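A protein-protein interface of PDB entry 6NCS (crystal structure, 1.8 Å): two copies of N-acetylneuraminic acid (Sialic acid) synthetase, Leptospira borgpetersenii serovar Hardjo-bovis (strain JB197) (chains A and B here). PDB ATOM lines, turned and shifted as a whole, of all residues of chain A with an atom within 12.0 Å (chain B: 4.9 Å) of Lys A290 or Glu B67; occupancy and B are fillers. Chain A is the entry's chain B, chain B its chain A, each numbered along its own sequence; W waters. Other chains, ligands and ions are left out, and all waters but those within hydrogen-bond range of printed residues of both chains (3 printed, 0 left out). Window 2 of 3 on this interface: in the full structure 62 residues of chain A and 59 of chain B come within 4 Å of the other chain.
The guanidinium group of Arg A288 lies within salt-bridge range of the side-chain carboxylate of Glu B67.
The side-chain amino group of Lys A290 is in salt-bridge range of the side-chain carboxylate of Glu B67 (2.9 Å).
OH of Tyr A283 is in hydrogen-bond range of O of Arg B68 (2.6 Å).
NH2 of Arg A288 sits at hydrogen-bond distance from O of Phe B108 (2.7 Å).
The side-chain sulfur (SG) of Cys B132 sits at hydrogen-bond distance from the guanidinium group (NH1) of Arg A284 (3.7 Å).
The side-chain amide oxygen (OD1) of Asn B133 lies close to the chain-end carboxylate (O) of Lys A290 (3.4 Å).
The backbone NH of Ile B134 is in hydrogen-bond range of the chain-end carboxylate of Lys A290, at 2.9 Å.
The chain-end carboxylate of Lys A290 lies within hydrogen-bond range of the side-chain hydroxyl of Thr B135, 2.5 Å away.
Water W2 lies within hydrogen-bond range of the side-chain carboxylate (OE2) of Glu B67 (2.7 Å), the backbone carbonyl oxygen (O) of Phe B108 (2.7 Å), the side-chain amide nitrogen (ND2) of Asn B133 (3.1 Å) and the guanidinium group (NH2) of Arg A288 (3.3 Å).
Water W3 lies within hydrogen-bond range of NE of Arg B68 (2.7 Å) and OH of Tyr A283 (3.0 Å).
Water W1 lies within hydrogen-bond range of N of Cys B132, O of Arg A288 and N of Asn B133.
No position is printed for both chains.
Tyr A283 touches Phe B69 (OH to CE1, 3.9 Å).
Leu A287 touches Phe B69 (CD1 to O, 3.6 Å).
Arg B68 touches Arg A288 (CA to NH1, 3.7 Å).
Cys B132 touches Arg A288.
CA of Asn B133 touches O of Arg A288, at 3.3 Å.
CA of Arg A289 touches O of Cys B132, 3.6 Å away.
Lys A290 touches four residues of chain B.
No residue of chain A comes within 4 Å of Asn B64.
No residue of chain A comes within 4 Å of Ser B65.
No residue of chain A comes within 4 Å of Glu B66.
No residue of chain A comes within 4 Å of Gly B70.
No residue of chain A comes within 4 Å of Asp B109.
Of chain A, only Arg A288 (3.3 Å) and Lys A290 (3.4 Å) come within 4 Å of Asn B133.
Ile B134 touches one residue of chain A.
Thr B135 touches just one residue of chain A: Lys A290 (2.5 Å).
Of the printed residues of chain B, Tyr A283 touches Arg B68 (2.6 Å) and Phe B69 (3.9 Å).
Printed residues of chain A within 4 Å of Cys B132: Arg A284 (3.7 Å), Arg A288 (3.7 Å) and Arg A289 (3.6 Å).
Of the printed residues of chain B, Leu A287 touches Phe B69 (3.6 Å).
Of the printed residues of chain A, Phe B69 touches Tyr A283 and Leu A287.
Of the 13 printed residues of chain B, 8 touch a printed residue of chain A.
Along chain B the printed residues that touch a printed residue of chain A span positions 67 to 135.
The side-chain amide oxygen (OD1) of Asn B64 sits at hydrogen-bond distance from the backbone NH (N) of Glu B67.
The backbone carbonyl oxygen of Tyr A283 is in hydrogen-bond range of the side-chain hydroxyl of Ser A286, 3.0 Å away.
OD1 of Asn A285 is in hydrogen-bond range of NE of Arg A284 (3.0 Å).
The backbone carbonyl oxygen of Asn A285 lies within hydrogen-bond range of the guanidinium group of Arg A289 (3.5 Å).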
ATOM      1  N   GLU A 280     -15.433 -16.736  -7.801  1.00  0.00           N
ATOM      2  CA  GLU A 280     -16.617 -16.154  -8.419  1.00  0.00           C
ATOM      3  C   GLU A 280     -17.618 -17.226  -8.829  1.00  0.00           C
ATOM      4  O   GLU A 280     -18.832 -16.987  -8.790  1.00  0.00           O
ATOM      5  CB  GLU A 280     -16.212 -15.301  -9.619  1.00  0.00           C
ATOM      6  CG  GLU A 280     -17.341 -14.432 -10.165  1.00  0.00           C
ATOM      7  CD  GLU A 280     -17.619 -13.208  -9.308  1.00  0.00           C
ATOM      8  OE1 GLU A 280     -18.555 -12.450  -9.648  1.00  0.00           O
ATOM      9  OE2 GLU A 280     -16.904 -12.998  -8.305  1.00  0.00           O
ATOM     10  N   ILE A 281     -17.129 -18.408  -9.219  1.00  0.00           N
ATOM     11  CA  ILE A 281     -18.015 -19.534  -9.505  1.00  0.00           C
ATOM     12  C   ILE A 281     -18.810 -19.922  -8.265  1.00  0.00           C
ATOM     13  O   ILE A 281     -20.018 -20.170  -8.339  1.00  0.00           O
ATOM     14  CB  ILE A 281     -17.207 -20.727 -10.049  1.00  0.00           C
ATOM     15  CG1 ILE A 281     -16.691 -20.419 -11.462  1.00  0.00           C
ATOM     16  CG2 ILE A 281     -18.061 -21.988 -10.039  1.00  0.00           C
ATOM     17  CD1 ILE A 281     -15.644 -21.394 -11.959  1.00  0.00           C
ATOM     18  N   GLU A 282     -18.146 -19.992  -7.106  1.00  0.00           N
ATOM     19  CA  GLU A 282     -18.844 -20.386  -5.883  1.00  0.00           C
ATOM     20  C   GLU A 282     -19.867 -19.338  -5.466  1.00  0.00           C
ATOM     21  O   GLU A 282     -20.961 -19.679  -4.998  1.00  0.00           O
ATOM     22  CB  GLU A 282     -17.843 -20.627  -4.759  1.00  0.00           C
ATOM     23  CG  GLU A 282     -16.930 -21.798  -5.012  1.00  0.00           C
ATOM     24  CD  GLU A 282     -15.886 -21.967  -3.932  1.00  0.00           C
ATOM     25  OE1 GLU A 282     -16.115 -21.496  -2.796  1.00  0.00           O
ATOM     26  OE2 GLU A 282     -14.831 -22.567  -4.227  1.00  0.00           O
ATOM     27  N   TYR A 283     -19.520 -18.059  -5.606  1.00  0.00           N
ATOM     28  CA  TYR A 283     -20.494 -16.998  -5.384  1.00  0.00           C
ATOM     29  C   TYR A 283     -21.686 -17.159  -6.320  1.00  0.00           C
ATOM     30  O   TYR A 283     -22.844 -17.136  -5.883  1.00  0.00           O
ATOM     31  CB  TYR A 283     -19.824 -15.638  -5.579  1.00  0.00           C
ATOM     32  CG  TYR A 283     -20.786 -14.495  -5.786  1.00  0.00           C
ATOM     33  CD1 TYR A 283     -21.644 -14.090  -4.772  1.00  0.00           C
ATOM     34  CD2 TYR A 283     -20.830 -13.814  -6.994  1.00  0.00           C
ATOM     35  CE1 TYR A 283     -22.530 -13.045  -4.965  1.00  0.00           C
ATOM     36  CE2 TYR A 283     -21.698 -12.766  -7.190  1.00  0.00           C
ATOM     37  CZ  TYR A 283     -22.547 -12.384  -6.174  1.00  0.00           C
ATOM     38  OH  TYR A 283     -23.414 -11.342  -6.379  1.00  0.00           O
ATOM     39  N   ARG A 284     -21.412 -17.337  -7.617  1.00  0.00           N
ATOM     40  CA  ARG A 284     -22.478 -17.490  -8.604  1.00  0.00           C
ATOM     41  C   ARG A 284     -23.394 -18.658  -8.253  1.00  0.00           C
ATOM     42  O   ARG A 284     -24.625 -18.533  -8.287  1.00  0.00           O
ATOM     43  CB  ARG A 284     -21.859 -17.679  -9.994  1.00  0.00           C
ATOM     44  CG  ARG A 284     -22.852 -17.884 -11.121  1.00  0.00           C
ATOM     45  CD  ARG A 284     -22.176 -18.549 -12.318  1.00  0.00           C
ATOM     46  NE  ARG A 284     -21.965 -19.978 -12.092  1.00  0.00           N
ATOM     47  CZ  ARG A 284     -21.447 -20.807 -12.994  1.00  0.00           C
ATOM     48  NH1 ARG A 284     -21.073 -20.342 -14.181  1.00  0.00           N
ATOM     49  NH2 ARG A 284     -21.304 -22.099 -12.712  1.00  0.00           N
ATOM     50  N   ASN A 285     -22.810 -19.807  -7.904  1.00  0.00           N
ATOM     51  CA  ASN A 285     -23.616 -20.997  -7.664  1.00  0.00           C
ATOM     52  C   ASN A 285     -24.426 -20.904  -6.378  1.00  0.00           C
ATOM     53  O   ASN A 285     -25.446 -21.590  -6.252  1.00  0.00           O
ATOM     54  CB  ASN A 285     -22.722 -22.240  -7.644  1.00  0.00           C
ATOM     55  CG  ASN A 285     -22.162 -22.572  -9.016  1.00  0.00           C
ATOM     56  OD1 ASN A 285     -22.609 -22.026 -10.031  1.00  0.00           O
ATOM     57  ND2 ASN A 285     -21.181 -23.467  -9.059  1.00  0.00           N
ATOM     58  N   SER A 286     -24.010 -20.069  -5.431  1.00  0.00           N
ATOM     59  CA  SER A 286     -24.698 -20.007  -4.148  1.00  0.00           C
ATOM     60  C   SER A 286     -25.823 -18.980  -4.124  1.00  0.00           C
ATOM     61  O   SER A 286     -26.790 -19.157  -3.378  1.00  0.00           O
ATOM     62  CB  SER A 286     -23.700 -19.694  -3.029  1.00  0.00           C
ATOM     63  OG  SER A 286     -23.248 -18.354  -3.127  1.00  0.00           O
ATOM     64  N   LEU A 287     -25.735 -17.920  -4.922  1.00  0.00           N
ATOM     65  CA  LEU A 287     -26.672 -16.806  -4.808  1.00  0.00           C
ATOM     66  C   LEU A 287     -27.295 -16.349  -6.117  1.00  0.00           C
ATOM     67  O   LEU A 287     -28.332 -15.676  -6.075  1.00  0.00           O
ATOM     68  CB  LEU A 287     -25.982 -15.595  -4.166  1.00  0.00           C
ATOM     69  CG  LEU A 287     -25.666 -15.723  -2.680  1.00  0.00           C
ATOM     70  CD1 LEU A 287     -24.622 -14.698  -2.262  1.00  0.00           C
ATOM     71  CD2 LEU A 287     -26.942 -15.546  -1.883  1.00  0.00           C
ATOM     72  N   ARG A 288     -26.711 -16.666  -7.266  1.00  0.00           N
ATOM     73  CA  ARG A 288     -27.150 -16.067  -8.519  1.00  0.00           C
ATOM     74  C   ARG A 288     -27.803 -17.073  -9.459  1.00  0.00           C
ATOM     75  O   ARG A 288     -28.081 -16.735 -10.612  1.00  0.00           O
ATOM     76  CB  ARG A 288     -25.968 -15.372  -9.206  1.00  0.00           C
ATOM     77  CG  ARG A 288     -25.200 -14.417  -8.295  1.00  0.00           C
ATOM     78  CD  ARG A 288     -26.133 -13.334  -7.712  1.00  0.00           C
ATOM     79  NE  ARG A 288     -26.623 -12.419  -8.746  1.00  0.00           N
ATOM     80  CZ  ARG A 288     -27.535 -11.470  -8.545  1.00  0.00           C
ATOM     81  NH1 ARG A 288     -28.081 -11.310  -7.343  1.00  0.00           N
ATOM     82  NH2 ARG A 288     -27.908 -10.687  -9.550  1.00  0.00           N
ATOM     83  N   ARG A 289     -28.066 -18.296  -9.003  1.00  0.00           N
ATOM     84  CA  ARG A 289     -28.758 -19.286  -9.831  1.00  0.00           C
ATOM     85  C   ARG A 289     -30.236 -19.235  -9.461  1.00  0.00           C
ATOM     86  O   ARG A 289     -30.768 -20.090  -8.751  1.00  0.00           O
ATOM     87  CB  ARG A 289     -28.149 -20.673  -9.652  1.00  0.00           C
ATOM     88  CG  ARG A 289     -26.693 -20.740 -10.091  1.00  0.00           C
ATOM     89  CD  ARG A 289     -26.233 -22.170 -10.338  1.00  0.00           C
ATOM     90  NE  ARG A 289     -26.564 -23.054  -9.225  1.00  0.00           N
ATOM     91  CZ  ARG A 289     -26.107 -24.296  -9.095  1.00  0.00           C
ATOM     92  NH1 ARG A 289     -25.286 -24.802 -10.008  1.00  0.00           N
ATOM     93  NH2 ARG A 289     -26.467 -25.031  -8.049  1.00  0.00           N
ATOM     94  N   LYS A 290     -30.899 -18.196  -9.954  1.00  0.00           N
ATOM     95  CA  LYS A 290     -32.290 -17.927  -9.614  1.00  0.00           C
ATOM     96  C   LYS A 290     -33.100 -17.594 -10.862  1.00  0.00           C
ATOM     97  O   LYS A 290     -32.584 -17.648 -11.979  1.00  0.00           O
ATOM     98  CB  LYS A 290     -32.380 -16.781  -8.597  1.00  0.00           C
ATOM     99  CG  LYS A 290     -31.675 -15.499  -9.026  1.00  0.00           C
ATOM    100  CD  LYS A 290     -31.084 -14.747  -7.828  1.00  0.00           C
ATOM    101  CE  LYS A 290     -32.160 -14.119  -6.961  1.00  0.00           C
ATOM    102  NZ  LYS A 290     -31.597 -13.493  -5.731  1.00  0.00           N
ATOM    103  OXT LYS A 290     -34.288 -17.275 -10.776  1.00  0.00           O
ATOM    104  N   ASN B  64     -29.549  -3.903  -5.843  1.00  0.00           N
ATOM    105  CA  ASN B  64     -29.802  -3.844  -4.410  1.00  0.00           C
ATOM    106  C   ASN B  64     -28.732  -4.675  -3.711  1.00  0.00           C
ATOM    107  O   ASN B  64     -28.527  -5.845  -4.057  1.00  0.00           O
ATOM    108  CB  ASN B  64     -31.202  -4.367  -4.082  1.00  0.00           C
ATOM    109  CG  ASN B  64     -31.431  -4.530  -2.590  1.00  0.00           C
ATOM    110  OD1 ASN B  64     -31.307  -5.626  -2.048  1.00  0.00           O
ATOM    111  ND2 ASN B  64     -31.775  -3.431  -1.919  1.00  0.00           N
ATOM    112  N   SER B  65     -28.040  -4.064  -2.744  1.00  0.00           N
ATOM    113  CA  SER B  65     -26.885  -4.709  -2.117  1.00  0.00           C
ATOM    114  C   SER B  65     -27.253  -6.053  -1.497  1.00  0.00           C
ATOM    115  O   SER B  65     -26.551  -7.053  -1.698  1.00  0.00           O
ATOM    116  CB  SER B  65     -26.287  -3.785  -1.055  1.00  0.00           C
ATOM    117  OG  SER B  65     -25.864  -2.558  -1.629  1.00  0.00           O
ATOM    118  N   GLU B  66     -28.339  -6.087  -0.716  1.00  0.00           N
ATOM    119  CA  GLU B  66     -28.735  -7.320  -0.040  1.00  0.00           C
ATOM    120  C   GLU B  66     -29.133  -8.406  -1.037  1.00  0.00           C
ATOM    121  O   GLU B  66     -28.823  -9.587  -0.841  1.00  0.00           O
ATOM    122  CB  GLU B  66     -29.882  -7.038   0.930  1.00  0.00           C
ATOM    123  CG  GLU B  66     -29.467  -6.271   2.176  1.00  0.00           C
ATOM    124  CD  GLU B  66     -29.485  -4.764   1.993  1.00  0.00           C
ATOM    125  OE1 GLU B  66     -29.714  -4.288   0.859  1.00  0.00           O
ATOM    126  OE2 GLU B  66     -29.281  -4.052   3.000  1.00  0.00           O
ATOM    127  N   GLU B  67     -29.837  -8.030  -2.105  1.00  0.00           N
ATOM    128  CA  GLU B  67     -30.176  -9.001  -3.136  1.00  0.00           C
ATOM    129  C   GLU B  67     -28.912  -9.552  -3.783  1.00  0.00           C
ATOM    130  O   GLU B  67     -28.807 -10.754  -4.065  1.00  0.00           O
ATOM    131  CB  GLU B  67     -31.078  -8.337  -4.178  1.00  0.00           C
ATOM    132  CG  GLU B  67     -31.822  -9.284  -5.096  1.00  0.00           C
ATOM    133  CD  GLU B  67     -30.978  -9.797  -6.247  1.00  0.00           C
ATOM    134  OE1 GLU B  67     -29.941  -9.172  -6.577  1.00  0.00           O
ATOM    135  OE2 GLU B  67     -31.364 -10.839  -6.827  1.00  0.00           O
ATOM    136  N   ARG B  68     -27.928  -8.686  -3.992  1.00  0.00           N
ATOM    137  CA  ARG B  68     -26.749  -9.061  -4.756  1.00  0.00           C
ATOM    138  C   ARG B  68     -25.802  -9.934  -3.939  1.00  0.00           C
ATOM    139  O   ARG B  68     -25.184 -10.859  -4.481  1.00  0.00           O
ATOM    140  CB  ARG B  68     -26.045  -7.796  -5.233  1.00  0.00           C
ATOM    141  CG  ARG B  68     -24.830  -8.020  -6.100  1.00  0.00           C
ATOM    142  CD  ARG B  68     -24.318  -6.680  -6.570  1.00  0.00           C
ATOM    143  NE  ARG B  68     -23.087  -6.764  -7.343  1.00  0.00           N
ATOM    144  CZ  ARG B  68     -22.541  -5.722  -7.957  1.00  0.00           C
ATOM    145  NH1 ARG B  68     -23.126  -4.527  -7.875  1.00  0.00           N
ATOM    146  NH2 ARG B  68     -21.420  -5.868  -8.652  1.00  0.00           N
ATOM    147  N   PHE B  69     -25.667  -9.667  -2.636  1.00  0.00           N
ATOM    148  CA  PHE B  69     -24.647 -10.357  -1.854  1.00  0.00           C
ATOM    149  C   PHE B  69     -25.171 -11.161  -0.676  1.00  0.00           C
ATOM    150  O   PHE B  69     -24.385 -11.887  -0.058  1.00  0.00           O
ATOM    151  CB  PHE B  69     -23.586  -9.360  -1.363  1.00  0.00           C
ATOM    152  CG  PHE B  69     -22.722  -8.828  -2.465  1.00  0.00           C
ATOM    153  CD1 PHE B  69     -21.837  -9.667  -3.127  1.00  0.00           C
ATOM    154  CD2 PHE B  69     -22.818  -7.508  -2.871  1.00  0.00           C
ATOM    155  CE1 PHE B  69     -21.054  -9.193  -4.153  1.00  0.00           C
ATOM    156  CE2 PHE B  69     -22.039  -7.026  -3.898  1.00  0.00           C
ATOM    157  CZ  PHE B  69     -21.149  -7.870  -4.543  1.00  0.00           C
ATOM    158  N   GLY B  70     -26.456 -11.070  -0.356  1.00  0.00           N
ATOM    159  CA  GLY B  70     -27.043 -11.975   0.619  1.00  0.00           C
ATOM    160  C   GLY B  70     -26.412 -11.822   1.989  1.00  0.00           C
ATOM    161  O   GLY B  70     -26.364 -10.727   2.559  1.00  0.00           O
ATOM    162  N   PHE B 108     -28.992  -5.936 -11.796  1.00  0.00           N
ATOM    163  CA  PHE B 108     -28.711  -7.169 -11.082  1.00  0.00           C
ATOM    164  C   PHE B 108     -29.976  -7.869 -10.625  1.00  0.00           C
ATOM    165  O   PHE B 108     -29.892  -8.946 -10.034  1.00  0.00           O
ATOM    166  CB  PHE B 108     -27.785  -6.896  -9.889  1.00  0.00           C
ATOM    167  CG  PHE B 108     -26.349  -6.662 -10.288  1.00  0.00           C
ATOM    168  CD1 PHE B 108     -25.962  -5.469 -10.869  1.00  0.00           C
ATOM    169  CD2 PHE B 108     -25.394  -7.652 -10.100  1.00  0.00           C
ATOM    170  CE1 PHE B 108     -24.638  -5.257 -11.253  1.00  0.00           C
ATOM    171  CE2 PHE B 108     -24.066  -7.443 -10.482  1.00  0.00           C
ATOM    172  CZ  PHE B 108     -23.696  -6.250 -11.058  1.00  0.00           C
ATOM    173  N   ASP B 109     -31.143  -7.286 -10.890  1.00  0.00           N
ATOM    174  CA  ASP B 109     -32.411  -7.943 -10.618  1.00  0.00           C
ATOM    175  C   ASP B 109     -33.451  -7.362 -11.561  1.00  0.00           C
ATOM    176  O   ASP B 109     -33.188  -6.408 -12.295  1.00  0.00           O
ATOM    177  CB  ASP B 109     -32.827  -7.799  -9.145  1.00  0.00           C
ATOM    178  CG  ASP B 109     -32.929  -6.345  -8.674  1.00  0.00           C
ATOM    179  OD1 ASP B 109     -33.196  -5.431  -9.477  1.00  0.00           O
ATOM    180  OD2 ASP B 109     -32.761  -6.123  -7.456  1.00  0.00           O
ATOM    181  N   CYS B 132     -25.961 -17.645 -15.197  1.00  0.00           N
ATOM    182  CA  CYS B 132     -26.882 -18.707 -14.828  1.00  0.00           C
ATOM    183  C   CYS B 132     -28.099 -18.169 -14.091  1.00  0.00           C
ATOM    184  O   CYS B 132     -28.825 -18.945 -13.462  1.00  0.00           O
ATOM    185  CB  CYS B 132     -26.174 -19.753 -13.967  1.00  0.00           C
ATOM    186  SG  CYS B 132     -24.759 -20.502 -14.789  1.00  0.00           S
ATOM    187  N   ASN B 133     -28.332 -16.858 -14.155  1.00  0.00           N
ATOM    188  CA  ASN B 133     -29.485 -16.222 -13.514  1.00  0.00           C
ATOM    189  C   ASN B 133     -30.639 -16.232 -14.516  1.00  0.00           C
ATOM    190  O   ASN B 133     -30.897 -15.259 -15.228  1.00  0.00           O
ATOM    191  CB  ASN B 133     -29.111 -14.811 -13.074  1.00  0.00           C
ATOM    192  CG  ASN B 133     -30.143 -14.164 -12.167  1.00  0.00           C
ATOM    193  OD1 ASN B 133     -31.331 -14.481 -12.217  1.00  0.00           O
ATOM    194  ND2 ASN B 133     -29.684 -13.237 -11.330  1.00  0.00           N
ATOM    195  N   ILE B 134     -31.344 -17.366 -14.568  1.00  0.00           N
ATOM    196  CA  ILE B 134     -32.308 -17.603 -15.645  1.00  0.00           C
ATOM    197  C   ILE B 134     -33.417 -16.558 -15.623  1.00  0.00           C
ATOM    198  O   ILE B 134     -33.820 -16.036 -16.670  1.00  0.00           O
ATOM    199  CB  ILE B 134     -32.880 -19.030 -15.548  1.00  0.00           C
ATOM    200  CG1 ILE B 134     -31.746 -20.054 -15.532  1.00  0.00           C
ATOM    201  CG2 ILE B 134     -33.832 -19.299 -16.714  1.00  0.00           C
ATOM    202  CD1 ILE B 134     -30.838 -19.972 -16.741  1.00  0.00           C
ATOM    203  N   THR B 135     -33.924 -16.233 -14.434  1.00  0.00           N
ATOM    204  CA  THR B 135     -34.983 -15.235 -14.332  1.00  0.00           C
ATOM    205  C   THR B 135     -34.539 -13.898 -14.919  1.00  0.00           C
ATOM    206  O   THR B 135     -35.282 -13.258 -15.672  1.00  0.00           O
ATOM    207  CB  THR B 135     -35.406 -15.069 -12.872  1.00  0.00           C
ATOM    208  OG1 THR B 135     -35.976 -16.295 -12.399  1.00  0.00           O
ATOM    209  CG2 THR B 135     -36.432 -13.956 -12.737  1.00  0.00           C
HETATM  210  O   HOH W   1     -25.758 -16.878 -12.415  1.00  0.00           O
HETATM  211  O   HOH W   2     -31.188 -11.269  -9.499  1.00  0.00           O
HETATM  212  O   HOH W   3     -21.932  -9.206  -7.854  1.00  0.00           O
